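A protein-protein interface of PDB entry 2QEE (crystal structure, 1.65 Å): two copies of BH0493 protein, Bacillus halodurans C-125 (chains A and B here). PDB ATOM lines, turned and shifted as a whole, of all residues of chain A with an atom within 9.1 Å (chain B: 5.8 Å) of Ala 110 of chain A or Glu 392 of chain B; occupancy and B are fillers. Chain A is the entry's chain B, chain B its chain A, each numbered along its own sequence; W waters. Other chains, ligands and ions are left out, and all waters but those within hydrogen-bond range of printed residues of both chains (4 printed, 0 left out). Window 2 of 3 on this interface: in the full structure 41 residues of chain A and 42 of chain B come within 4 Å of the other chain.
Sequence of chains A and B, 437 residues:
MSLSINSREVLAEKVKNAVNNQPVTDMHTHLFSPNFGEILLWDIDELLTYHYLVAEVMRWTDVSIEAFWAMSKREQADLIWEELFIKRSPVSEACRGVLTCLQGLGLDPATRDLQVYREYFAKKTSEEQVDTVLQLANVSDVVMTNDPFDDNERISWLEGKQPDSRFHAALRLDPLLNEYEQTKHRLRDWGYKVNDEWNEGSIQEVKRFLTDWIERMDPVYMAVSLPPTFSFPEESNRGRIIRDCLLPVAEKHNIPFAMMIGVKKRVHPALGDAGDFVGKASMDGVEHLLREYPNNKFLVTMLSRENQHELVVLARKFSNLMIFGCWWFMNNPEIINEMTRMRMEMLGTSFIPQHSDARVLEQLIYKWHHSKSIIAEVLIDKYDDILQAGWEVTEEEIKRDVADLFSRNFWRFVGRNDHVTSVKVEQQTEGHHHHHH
Ala 110 of chain A touches just these residues of chain B: Gly 390 (3.2 Å) and Glu 392 (3.6 Å). Glu 392 of chain B touches just these residues of chain A: Ala 110 and Arg 112. Val 393 of chain B touches none of the printed residues of chain A. Of the printed residues of chain A, Ile 386 of chain B touches Pro 90. Printed residues of chain A within 4 Å of Glu 397 of chain B: Arg 112 (2.9 Å). Printed residues of chain B within 4 Å of Pro 90 of chain A: Ile 386 and Trp 391. Printed residues of chain B within 4 Å of Arg 112 of chain A: Trp 391, Glu 392 and Glu 397. Of the printed residues of chain B, Trp 81 of chain A touches Trp 391 (3.8 Å). Leu 107 of chain A touches none of the printed residues of chain B. Thr 111 of chain A touches none of the printed residues of chain B. The nearest residue of chain B that does not touch Ala 110 of chain A is Trp 391 of chain B (4.6 Å). The nearest printed residue of chain B that does not touch Gln 103 of chain A is Leu 387 of chain B (5.2 Å).
Water W2 bridges the side-chain carboxylate (OD1) of Asp 108 of chain A and the backbone carbonyl oxygen (O) of Gly 390 of chain B. Water W3 lies within hydrogen-bond range of the side-chain carboxylate of Glu 397 of chain B (2.6 Å), the backbone carbonyl oxygen of Ile 86 of chain A (2.7 Å) and the guanidinium group of Arg 112 of chain A (3.5 Å). Water W4 lies within hydrogen-bond range of OG of Ser 89 of chain A (2.7 Å), OE1 of Glu 397 of chain B (2.8 Å) and NE1 of Trp 391 of chain B (3.0 Å). Water W1 lies within hydrogen-bond range of NE of Arg 112 of chain A (2.9 Å), O of Pro 109 of chain A (3.0 Å), N of Glu 392 of chain B (3.0 Å) and O of Ala 110 of chain A (3.2 Å).
The side-chain amide nitrogen of Gln 103 of chain A sits close to the backbone NH of Gly 390 of chain B (3.4 Å). The backbone NH of Ala 110 of chain A lies within hydrogen-bond range of the backbone carbonyl oxygen of Gly 390 of chain B (3.2 Å). NH2 of Arg 112 of chain A lies within hydrogen-bond range of O of Glu 392 of chain B, at 2.8 Å. OE2 of Glu 397 of chain B lies within salt-bridge range of NH1 of Arg 112 of chain A.
Of the 9 printed residues of chain B, 5 touch a printed residue of chain A. Along chain A the printed residues that touch a printed residue of chain B span positions 81 to 112. Among the printed residues, 13 pairs touch across the chains.
OE1 of Glu 392 of chain B is in hydrogen-bond range of OG of Ser 4 of chain B. The backbone NH (N) of Trp 391 of chain B sits at hydrogen-bond distance from the backbone carbonyl oxygen (O) of Ile 386 of chain B, 3.0 Å away. OG1 of Thr 394 of chain B is in hydrogen-bond range of N of Glu 397 of chain B. The backbone NH (N) of Ile 86 of chain A lies within hydrogen-bond range of the backbone carbonyl oxygen (O) of Trp 81 of chain A (3.2 Å). The backbone carbonyl oxygen of Pro 109 of chain A lies close to the side-chain hydroxyl of Tyr 117 of chain A, at 3.4 Å. The backbone NH of Arg 112 of chain A is in hydrogen-bond range of the side-chain hydroxyl of Tyr 117 of chain A (3.1 Å).
No position is printed for both chains. Of the 13 pairs that touch across the chains among the printed residues, none has its exchanged pair printed and touching as well.
Trp 81 of chain A touches Trp 391 of chain B. O of Phe 85 of chain A touches CZ2 of Trp 391 of chain B (3.3 Å). CG2 of Ile 386 of chain B touches O of Pro 90 of chain A (3.2 Å). CD of Pro 90 of chain A touches NE1 of Trp 391 of chain B (3.6 Å). CD2 of Leu 99 of chain A touches CE3 of Trp 391 of chain B, at 3.7 Å. Gly 390 of chain B touches Pro 109 of chain A (O to C, 3.8 Å). Pro 109 of chain A touches Trp 391 of chain B (O to CE3, 3.6 Å). CG of Glu 392 of chain B touches CB of Ala 110 of chain A, 3.6 Å away. Trp 391 of chain B touches Arg 112 of chain A (CZ2 to NE, 3.4 Å).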
ATOM      1  N   TRP A  81      32.311   2.217 -35.433  1.00  0.00           N
ATOM      2  CA  TRP A  81      31.001   2.036 -34.807  1.00  0.00           C
ATOM      3  C   TRP A  81      30.698   0.557 -34.666  1.00  0.00           C
ATOM      4  O   TRP A  81      30.357   0.074 -33.564  1.00  0.00           O
ATOM      5  CB  TRP A  81      29.914   2.768 -35.646  1.00  0.00           C
ATOM      6  CG  TRP A  81      28.544   2.719 -35.083  1.00  0.00           C
ATOM      7  CD1 TRP A  81      27.507   1.930 -35.511  1.00  0.00           C
ATOM      8  CD2 TRP A  81      28.024   3.492 -33.976  1.00  0.00           C
ATOM      9  NE1 TRP A  81      26.396   2.148 -34.726  1.00  0.00           N
ATOM     10  CE2 TRP A  81      26.668   3.128 -33.814  1.00  0.00           C
ATOM     11  CE3 TRP A  81      28.567   4.476 -33.137  1.00  0.00           C
ATOM     12  CZ2 TRP A  81      25.843   3.689 -32.825  1.00  0.00           C
ATOM     13  CZ3 TRP A  81      27.755   5.027 -32.155  1.00  0.00           C
ATOM     14  CH2 TRP A  81      26.389   4.643 -32.020  1.00  0.00           C
ATOM     15  N   PHE A  85      31.116  -0.469 -30.769  1.00  0.00           N
ATOM     16  CA  PHE A  85      29.814  -0.196 -30.204  1.00  0.00           C
ATOM     17  C   PHE A  85      28.830  -1.343 -30.404  1.00  0.00           C
ATOM     18  O   PHE A  85      27.995  -1.623 -29.560  1.00  0.00           O
ATOM     19  CB  PHE A  85      29.251   1.101 -30.818  1.00  0.00           C
ATOM     20  CG  PHE A  85      30.028   2.350 -30.447  1.00  0.00           C
ATOM     21  CD1 PHE A  85      29.517   3.251 -29.500  1.00  0.00           C
ATOM     22  CD2 PHE A  85      31.261   2.623 -31.052  1.00  0.00           C
ATOM     23  CE1 PHE A  85      30.231   4.429 -29.162  1.00  0.00           C
ATOM     24  CE2 PHE A  85      31.995   3.782 -30.739  1.00  0.00           C
ATOM     25  CZ  PHE A  85      31.485   4.700 -29.802  1.00  0.00           C
ATOM     26  N   ILE A  86      28.906  -1.973 -31.574  1.00  0.00           N
ATOM     27  CA  ILE A  86      27.994  -3.074 -31.914  1.00  0.00           C
ATOM     28  C   ILE A  86      28.490  -4.480 -31.523  1.00  0.00           C
ATOM     29  O   ILE A  86      27.753  -5.237 -30.883  1.00  0.00           O
ATOM     30  CB  ILE A  86      27.626  -3.013 -33.437  1.00  0.00           C
ATOM     31  CG1 ILE A  86      27.141  -1.597 -33.814  1.00  0.00           C
ATOM     32  CG2 ILE A  86      26.605  -4.062 -33.744  1.00  0.00           C
ATOM     33  CD1 ILE A  86      26.004  -0.985 -32.938  1.00  0.00           C
ATOM     34  N   SER A  89      30.333  -4.016 -26.219  1.00  0.00           N
ATOM     35  CA  SER A  89      29.698  -2.824 -25.578  1.00  0.00           C
ATOM     36  C   SER A  89      30.698  -1.690 -25.492  1.00  0.00           C
ATOM     37  O   SER A  89      31.841  -1.917 -25.107  1.00  0.00           O
ATOM     38  CB  SER A  89      29.105  -3.115 -24.202  1.00  0.00           C
ATOM     39  OG  SER A  89      28.083  -4.110 -24.247  1.00  0.00           O
ATOM     40  N   PRO A  90      30.253  -0.439 -25.806  1.00  0.00           N
ATOM     41  CA  PRO A  90      31.093   0.756 -25.843  1.00  0.00           C
ATOM     42  C   PRO A  90      31.388   1.282 -24.431  1.00  0.00           C
ATOM     43  O   PRO A  90      31.061   2.426 -24.100  1.00  0.00           O
ATOM     44  CB  PRO A  90      30.219   1.800 -26.566  1.00  0.00           C
ATOM     45  CG  PRO A  90      28.797   1.356 -26.397  1.00  0.00           C
ATOM     46  CD  PRO A  90      28.853  -0.176 -26.233  1.00  0.00           C
ATOM     47  N   LEU A  99      28.855   8.657 -26.866  1.00  0.00           N
ATOM     48  CA  LEU A  99      27.449   8.537 -26.472  1.00  0.00           C
ATOM     49  C   LEU A  99      26.981   9.779 -25.693  1.00  0.00           C
ATOM     50  O   LEU A  99      25.882  10.309 -25.938  1.00  0.00           O
ATOM     51  CB  LEU A  99      27.205   7.243 -25.681  1.00  0.00           C
ATOM     52  CG  LEU A  99      27.676   6.003 -26.455  1.00  0.00           C
ATOM     53  CD1 LEU A  99      27.408   4.752 -25.601  1.00  0.00           C
ATOM     54  CD2 LEU A  99      27.007   5.877 -27.872  1.00  0.00           C
ATOM     55  N   LEU A 102      26.316  12.518 -28.194  1.00  0.00           N
ATOM     56  CA  LEU A 102      25.038  12.280 -28.919  1.00  0.00           C
ATOM     57  C   LEU A 102      23.832  12.639 -28.066  1.00  0.00           C
ATOM     58  O   LEU A 102      22.966  13.427 -28.469  1.00  0.00           O
ATOM     59  CB  LEU A 102      24.979  10.796 -29.354  1.00  0.00           C
ATOM     60  CG  LEU A 102      25.939  10.379 -30.464  1.00  0.00           C
ATOM     61  CD1 LEU A 102      25.842   8.858 -30.712  1.00  0.00           C
ATOM     62  CD2 LEU A 102      25.625  11.195 -31.813  1.00  0.00           C
ATOM     63  N   GLN A 103      23.805  12.150 -26.827  1.00  0.00           N
ATOM     64  CA  GLN A 103      22.705  12.412 -25.951  1.00  0.00           C
ATOM     65  C   GLN A 103      22.589  13.898 -25.673  1.00  0.00           C
ATOM     66  O   GLN A 103      21.485  14.450 -25.630  1.00  0.00           O
ATOM     67  CB  GLN A 103      22.914  11.641 -24.657  1.00  0.00           C
ATOM     68  CG  GLN A 103      21.765  11.765 -23.729  1.00  0.00           C
ATOM     69  CD  GLN A 103      22.099  11.240 -22.365  1.00  0.00           C
ATOM     70  OE1 GLN A 103      23.081  11.668 -21.736  1.00  0.00           O
ATOM     71  NE2 GLN A 103      21.285  10.326 -21.890  1.00  0.00           N
ATOM     72  N   LEU A 107      20.175  13.753 -29.559  1.00  0.00           N
ATOM     73  CA  LEU A 107      20.079  12.533 -30.341  1.00  0.00           C
ATOM     74  C   LEU A 107      19.877  11.347 -29.392  1.00  0.00           C
ATOM     75  O   LEU A 107      20.148  11.461 -28.204  1.00  0.00           O
ATOM     76  CB  LEU A 107      21.283  12.394 -31.277  1.00  0.00           C
ATOM     77  CG  LEU A 107      21.534  13.588 -32.227  1.00  0.00           C
ATOM     78  CD1 LEU A 107      22.913  13.613 -32.852  1.00  0.00           C
ATOM     79  CD2 LEU A 107      20.401  13.671 -33.306  1.00  0.00           C
ATOM     80  N   ASP A 108      19.337  10.239 -29.881  1.00  0.00           N
ATOM     81  CA  ASP A 108      19.028   9.147 -28.970  1.00  0.00           C
ATOM     82  C   ASP A 108      19.961   7.947 -29.226  1.00  0.00           C
ATOM     83  O   ASP A 108      19.806   7.237 -30.243  1.00  0.00           O
ATOM     84  CB  ASP A 108      17.558   8.751 -29.143  1.00  0.00           C
ATOM     85  CG  ASP A 108      17.086   7.768 -28.091  1.00  0.00           C
ATOM     86  OD1 ASP A 108      17.924   7.328 -27.281  1.00  0.00           O
ATOM     87  OD2 ASP A 108      15.874   7.445 -28.078  1.00  0.00           O
ATOM     88  N   PRO A 109      20.974   7.735 -28.341  1.00  0.00           N
ATOM     89  CA  PRO A 109      21.813   6.544 -28.548  1.00  0.00           C
ATOM     90  C   PRO A 109      21.090   5.216 -28.519  1.00  0.00           C
ATOM     91  O   PRO A 109      21.626   4.247 -29.008  1.00  0.00           O
ATOM     92  CB  PRO A 109      22.807   6.607 -27.374  1.00  0.00           C
ATOM     93  CG  PRO A 109      22.954   8.043 -27.101  1.00  0.00           C
ATOM     94  CD  PRO A 109      21.508   8.575 -27.254  1.00  0.00           C
ATOM     95  N   ALA A 110      19.919   5.155 -27.895  1.00  0.00           N
ATOM     96  CA  ALA A 110      19.181   3.895 -27.814  1.00  0.00           C
ATOM     97  C   ALA A 110      18.882   3.300 -29.200  1.00  0.00           C
ATOM     98  O   ALA A 110      18.915   2.087 -29.356  1.00  0.00           O
ATOM     99  CB  ALA A 110      17.908   4.075 -27.004  1.00  0.00           C
ATOM    100  N   THR A 111      18.635   4.139 -30.209  1.00  0.00           N
ATOM    101  CA  THR A 111      18.325   3.648 -31.563  1.00  0.00           C
ATOM    102  C   THR A 111      19.546   3.076 -32.310  1.00  0.00           C
ATOM    103  O   THR A 111      19.406   2.265 -33.258  1.00  0.00           O
ATOM    104  CB  THR A 111      17.675   4.756 -32.411  1.00  0.00           C
ATOM    105  OG1 THR A 111      18.620   5.819 -32.617  1.00  0.00           O
ATOM    106  CG2 THR A 111      16.450   5.268 -31.699  1.00  0.00           C
ATOM    107  N   ARG A 112      20.758   3.474 -31.896  1.00  0.00           N
ATOM    108  CA  ARG A 112      21.977   3.133 -32.639  1.00  0.00           C
ATOM    109  C   ARG A 112      21.953   3.617 -34.109  1.00  0.00           C
ATOM    110  O   ARG A 112      22.610   3.056 -34.982  1.00  0.00           O
ATOM    111  CB  ARG A 112      22.259   1.629 -32.548  1.00  0.00           C
ATOM    112  CG  ARG A 112      22.309   1.193 -31.065  1.00  0.00           C
ATOM    113  CD  ARG A 112      22.774  -0.228 -30.918  1.00  0.00           C
ATOM    114  NE  ARG A 112      22.626  -0.658 -29.531  1.00  0.00           N
ATOM    115  CZ  ARG A 112      22.977  -1.853 -29.105  1.00  0.00           C
ATOM    116  NH1 ARG A 112      23.439  -2.745 -29.979  1.00  0.00           N
ATOM    117  NH2 ARG A 112      22.822  -2.170 -27.814  1.00  0.00           N
ATOM    118  N   ASP A 113      21.198   4.677 -34.369  1.00  0.00           N
ATOM    119  CA  ASP A 113      20.876   5.027 -35.766  1.00  0.00           C
ATOM    120  C   ASP A 113      21.874   6.029 -36.313  1.00  0.00           C
ATOM    121  O   ASP A 113      21.608   7.246 -36.325  1.00  0.00           O
ATOM    122  CB  ASP A 113      19.452   5.571 -35.829  1.00  0.00           C
ATOM    123  CG  ASP A 113      18.886   5.514 -37.231  1.00  0.00           C
ATOM    124  OD1 ASP A 113      19.692   5.576 -38.167  1.00  0.00           O
ATOM    125  OD2 ASP A 113      17.655   5.393 -37.381  1.00  0.00           O
ATOM    126  N   LEU A 114      23.035   5.531 -36.735  1.00  0.00           N
ATOM    127  CA  LEU A 114      24.147   6.403 -37.098  1.00  0.00           C
ATOM    128  C   LEU A 114      23.783   7.341 -38.265  1.00  0.00           C
ATOM    129  O   LEU A 114      24.188   8.510 -38.313  1.00  0.00           O
ATOM    130  CB  LEU A 114      25.402   5.570 -37.416  1.00  0.00           C
ATOM    131  CG  LEU A 114      26.754   6.237 -37.639  1.00  0.00           C
ATOM    132  CD1 LEU A 114      27.131   7.234 -36.532  1.00  0.00           C
ATOM    133  CD2 LEU A 114      27.887   5.189 -37.925  1.00  0.00           C
ATOM    134  N   TYR A 117      21.854  10.183 -36.736  1.00  0.00           N
ATOM    135  CA  TYR A 117      22.871  11.058 -36.128  1.00  0.00           C
ATOM    136  C   TYR A 117      23.596  11.942 -37.174  1.00  0.00           C
ATOM    137  O   TYR A 117      23.775  13.133 -36.957  1.00  0.00           O
ATOM    138  CB  TYR A 117      23.910  10.245 -35.297  1.00  0.00           C
ATOM    139  CG  TYR A 117      23.342   9.204 -34.341  1.00  0.00           C
ATOM    140  CD1 TYR A 117      22.068   9.349 -33.784  1.00  0.00           C
ATOM    141  CD2 TYR A 117      24.109   8.086 -33.949  1.00  0.00           C
ATOM    142  CE1 TYR A 117      21.553   8.383 -32.922  1.00  0.00           C
ATOM    143  CE2 TYR A 117      23.603   7.129 -33.070  1.00  0.00           C
ATOM    144  CZ  TYR A 117      22.340   7.283 -32.565  1.00  0.00           C
ATOM    145  OH  TYR A 117      21.781   6.364 -31.711  1.00  0.00           O
ATOM    146  N   SER B   4      13.727  -4.164 -21.410  1.00  0.00           N
ATOM    147  CA  SER B   4      14.900  -3.290 -21.357  1.00  0.00           C
ATOM    148  C   SER B   4      15.440  -3.145 -19.931  1.00  0.00           C
ATOM    149  O   SER B   4      14.675  -3.169 -18.965  1.00  0.00           O
ATOM    150  CB  SER B   4      14.554  -1.911 -21.956  1.00  0.00           C
ATOM    151  OG  SER B   4      15.683  -1.051 -22.001  1.00  0.00           O
ATOM    152  N   ILE B 386      27.222   4.034 -19.382  1.00  0.00           N
ATOM    153  CA  ILE B 386      26.680   4.155 -20.757  1.00  0.00           C
ATOM    154  C   ILE B 386      25.140   4.109 -20.776  1.00  0.00           C
ATOM    155  O   ILE B 386      24.516   4.770 -21.627  1.00  0.00           O
ATOM    156  CB  ILE B 386      27.314   3.152 -21.771  1.00  0.00           C
ATOM    157  CG1 ILE B 386      27.125   1.691 -21.348  1.00  0.00           C
ATOM    158  CG2 ILE B 386      28.802   3.496 -22.023  1.00  0.00           C
ATOM    159  CD1 ILE B 386      27.653   0.737 -22.437  1.00  0.00           C
ATOM    160  N   LEU B 387      24.507   3.385 -19.857  1.00  0.00           N
ATOM    161  CA  LEU B 387      23.044   3.499 -19.695  1.00  0.00           C
ATOM    162  C   LEU B 387      22.633   4.954 -19.413  1.00  0.00           C
ATOM    163  O   LEU B 387      21.651   5.477 -19.986  1.00  0.00           O
ATOM    164  CB  LEU B 387      22.589   2.619 -18.547  1.00  0.00           C
ATOM    165  CG  LEU B 387      21.787   1.346 -18.791  1.00  0.00           C
ATOM    166  CD1 LEU B 387      22.195   0.690 -20.048  1.00  0.00           C
ATOM    167  CD2 LEU B 387      21.922   0.392 -17.611  1.00  0.00           C
ATOM    168  N   GLY B 390      22.278   7.062 -22.363  1.00  0.00           N
ATOM    169  CA  GLY B 390      21.203   6.707 -23.281  1.00  0.00           C
ATOM    170  C   GLY B 390      21.345   5.411 -24.023  1.00  0.00           C
ATOM    171  O   GLY B 390      20.430   4.997 -24.748  1.00  0.00           O
ATOM    172  N   TRP B 391      22.485   4.744 -23.887  1.00  0.00           N
ATOM    173  CA  TRP B 391      22.682   3.472 -24.570  1.00  0.00           C
ATOM    174  C   TRP B 391      21.814   2.396 -23.936  1.00  0.00           C
ATOM    175  O   TRP B 391      21.559   2.399 -22.717  1.00  0.00           O
ATOM    176  CB  TRP B 391      24.133   3.039 -24.456  1.00  0.00           C
ATOM    177  CG  TRP B 391      24.552   1.922 -25.315  1.00  0.00           C
ATOM    178  CD1 TRP B 391      24.823   0.627 -24.925  1.00  0.00           C
ATOM    179  CD2 TRP B 391      24.838   1.988 -26.710  1.00  0.00           C
ATOM    180  NE1 TRP B 391      25.261  -0.101 -25.994  1.00  0.00           N
ATOM    181  CE2 TRP B 391      25.270   0.694 -27.111  1.00  0.00           C
ATOM    182  CE3 TRP B 391      24.755   3.011 -27.666  1.00  0.00           C
ATOM    183  CZ2 TRP B 391      25.620   0.397 -28.422  1.00  0.00           C
ATOM    184  CZ3 TRP B 391      25.126   2.724 -28.959  1.00  0.00           C
ATOM    185  CH2 TRP B 391      25.538   1.424 -29.339  1.00  0.00           C
ATOM    186  N   GLU B 392      21.303   1.503 -24.772  1.00  0.00           N
ATOM    187  CA  GLU B 392      20.538   0.366 -24.240  1.00  0.00           C
ATOM    188  C   GLU B 392      21.390  -0.894 -24.317  1.00  0.00           C
ATOM    189  O   GLU B 392      21.705  -1.385 -25.404  1.00  0.00           O
ATOM    190  CB  GLU B 392      19.243   0.174 -25.027  1.00  0.00           C
ATOM    191  CG  GLU B 392      18.163   1.239 -24.752  1.00  0.00           C
ATOM    192  CD  GLU B 392      16.755   0.860 -25.285  1.00  0.00           C
ATOM    193  OE1 GLU B 392      15.774   1.123 -24.548  1.00  0.00           O
ATOM    194  OE2 GLU B 392      16.629   0.314 -26.417  1.00  0.00           O
ATOM    195  N   VAL B 393      21.778  -1.425 -23.171  1.00  0.00           N
ATOM    196  CA  VAL B 393      22.543  -2.674 -23.205  1.00  0.00           C
ATOM    197  C   VAL B 393      21.627  -3.872 -22.984  1.00  0.00           C
ATOM    198  O   VAL B 393      20.732  -3.818 -22.137  1.00  0.00           O
ATOM    199  CB  VAL B 393      23.897  -2.633 -22.364  1.00  0.00           C
ATOM    200  CG1 VAL B 393      24.121  -1.314 -21.654  1.00  0.00           C
ATOM    201  CG2 VAL B 393      24.135  -3.875 -21.526  1.00  0.00           C
ATOM    202  N   THR B 394      21.789  -4.929 -23.773  1.00  0.00           N
ATOM    203  CA  THR B 394      20.921  -6.102 -23.611  1.00  0.00           C
ATOM    204  C   THR B 394      21.601  -7.152 -22.743  1.00  0.00           C
ATOM    205  O   THR B 394      22.835  -7.181 -22.647  1.00  0.00           O
ATOM    206  CB  THR B 394      20.523  -6.754 -24.958  1.00  0.00           C
ATOM    207  OG1 THR B 394      21.663  -7.382 -25.562  1.00  0.00           O
ATOM    208  CG2 THR B 394      19.937  -5.687 -25.945  1.00  0.00           C
ATOM    209  N   GLU B 397      24.096  -8.946 -24.709  1.00  0.00           N
ATOM    210  CA  GLU B 397      25.358  -8.219 -24.918  1.00  0.00           C
ATOM    211  C   GLU B 397      26.271  -8.340 -23.688  1.00  0.00           C
ATOM    212  O   GLU B 397      27.453  -8.502 -23.851  1.00  0.00           O
ATOM    213  CB  GLU B 397      25.103  -6.778 -25.288  1.00  0.00           C
ATOM    214  CG  GLU B 397      24.574  -6.675 -26.796  1.00  0.00           C
ATOM    215  CD  GLU B 397      23.967  -5.353 -27.122  1.00  0.00           C
ATOM    216  OE1 GLU B 397      23.730  -4.565 -26.194  1.00  0.00           O
ATOM    217  OE2 GLU B 397      23.698  -5.127 -28.324  1.00  0.00           O
HETATM  218  O   HOH W   1      21.679   1.511 -27.793  1.00  0.00           O
HETATM  219  O   HOH W   2      18.287   6.757 -24.768  1.00  0.00           O
HETATM  220  O   HOH W   3      25.089  -5.740 -30.457  1.00  0.00           O
HETATM  221  O   HOH W   4      25.976  -3.034 -25.624  1.00  0.00           O
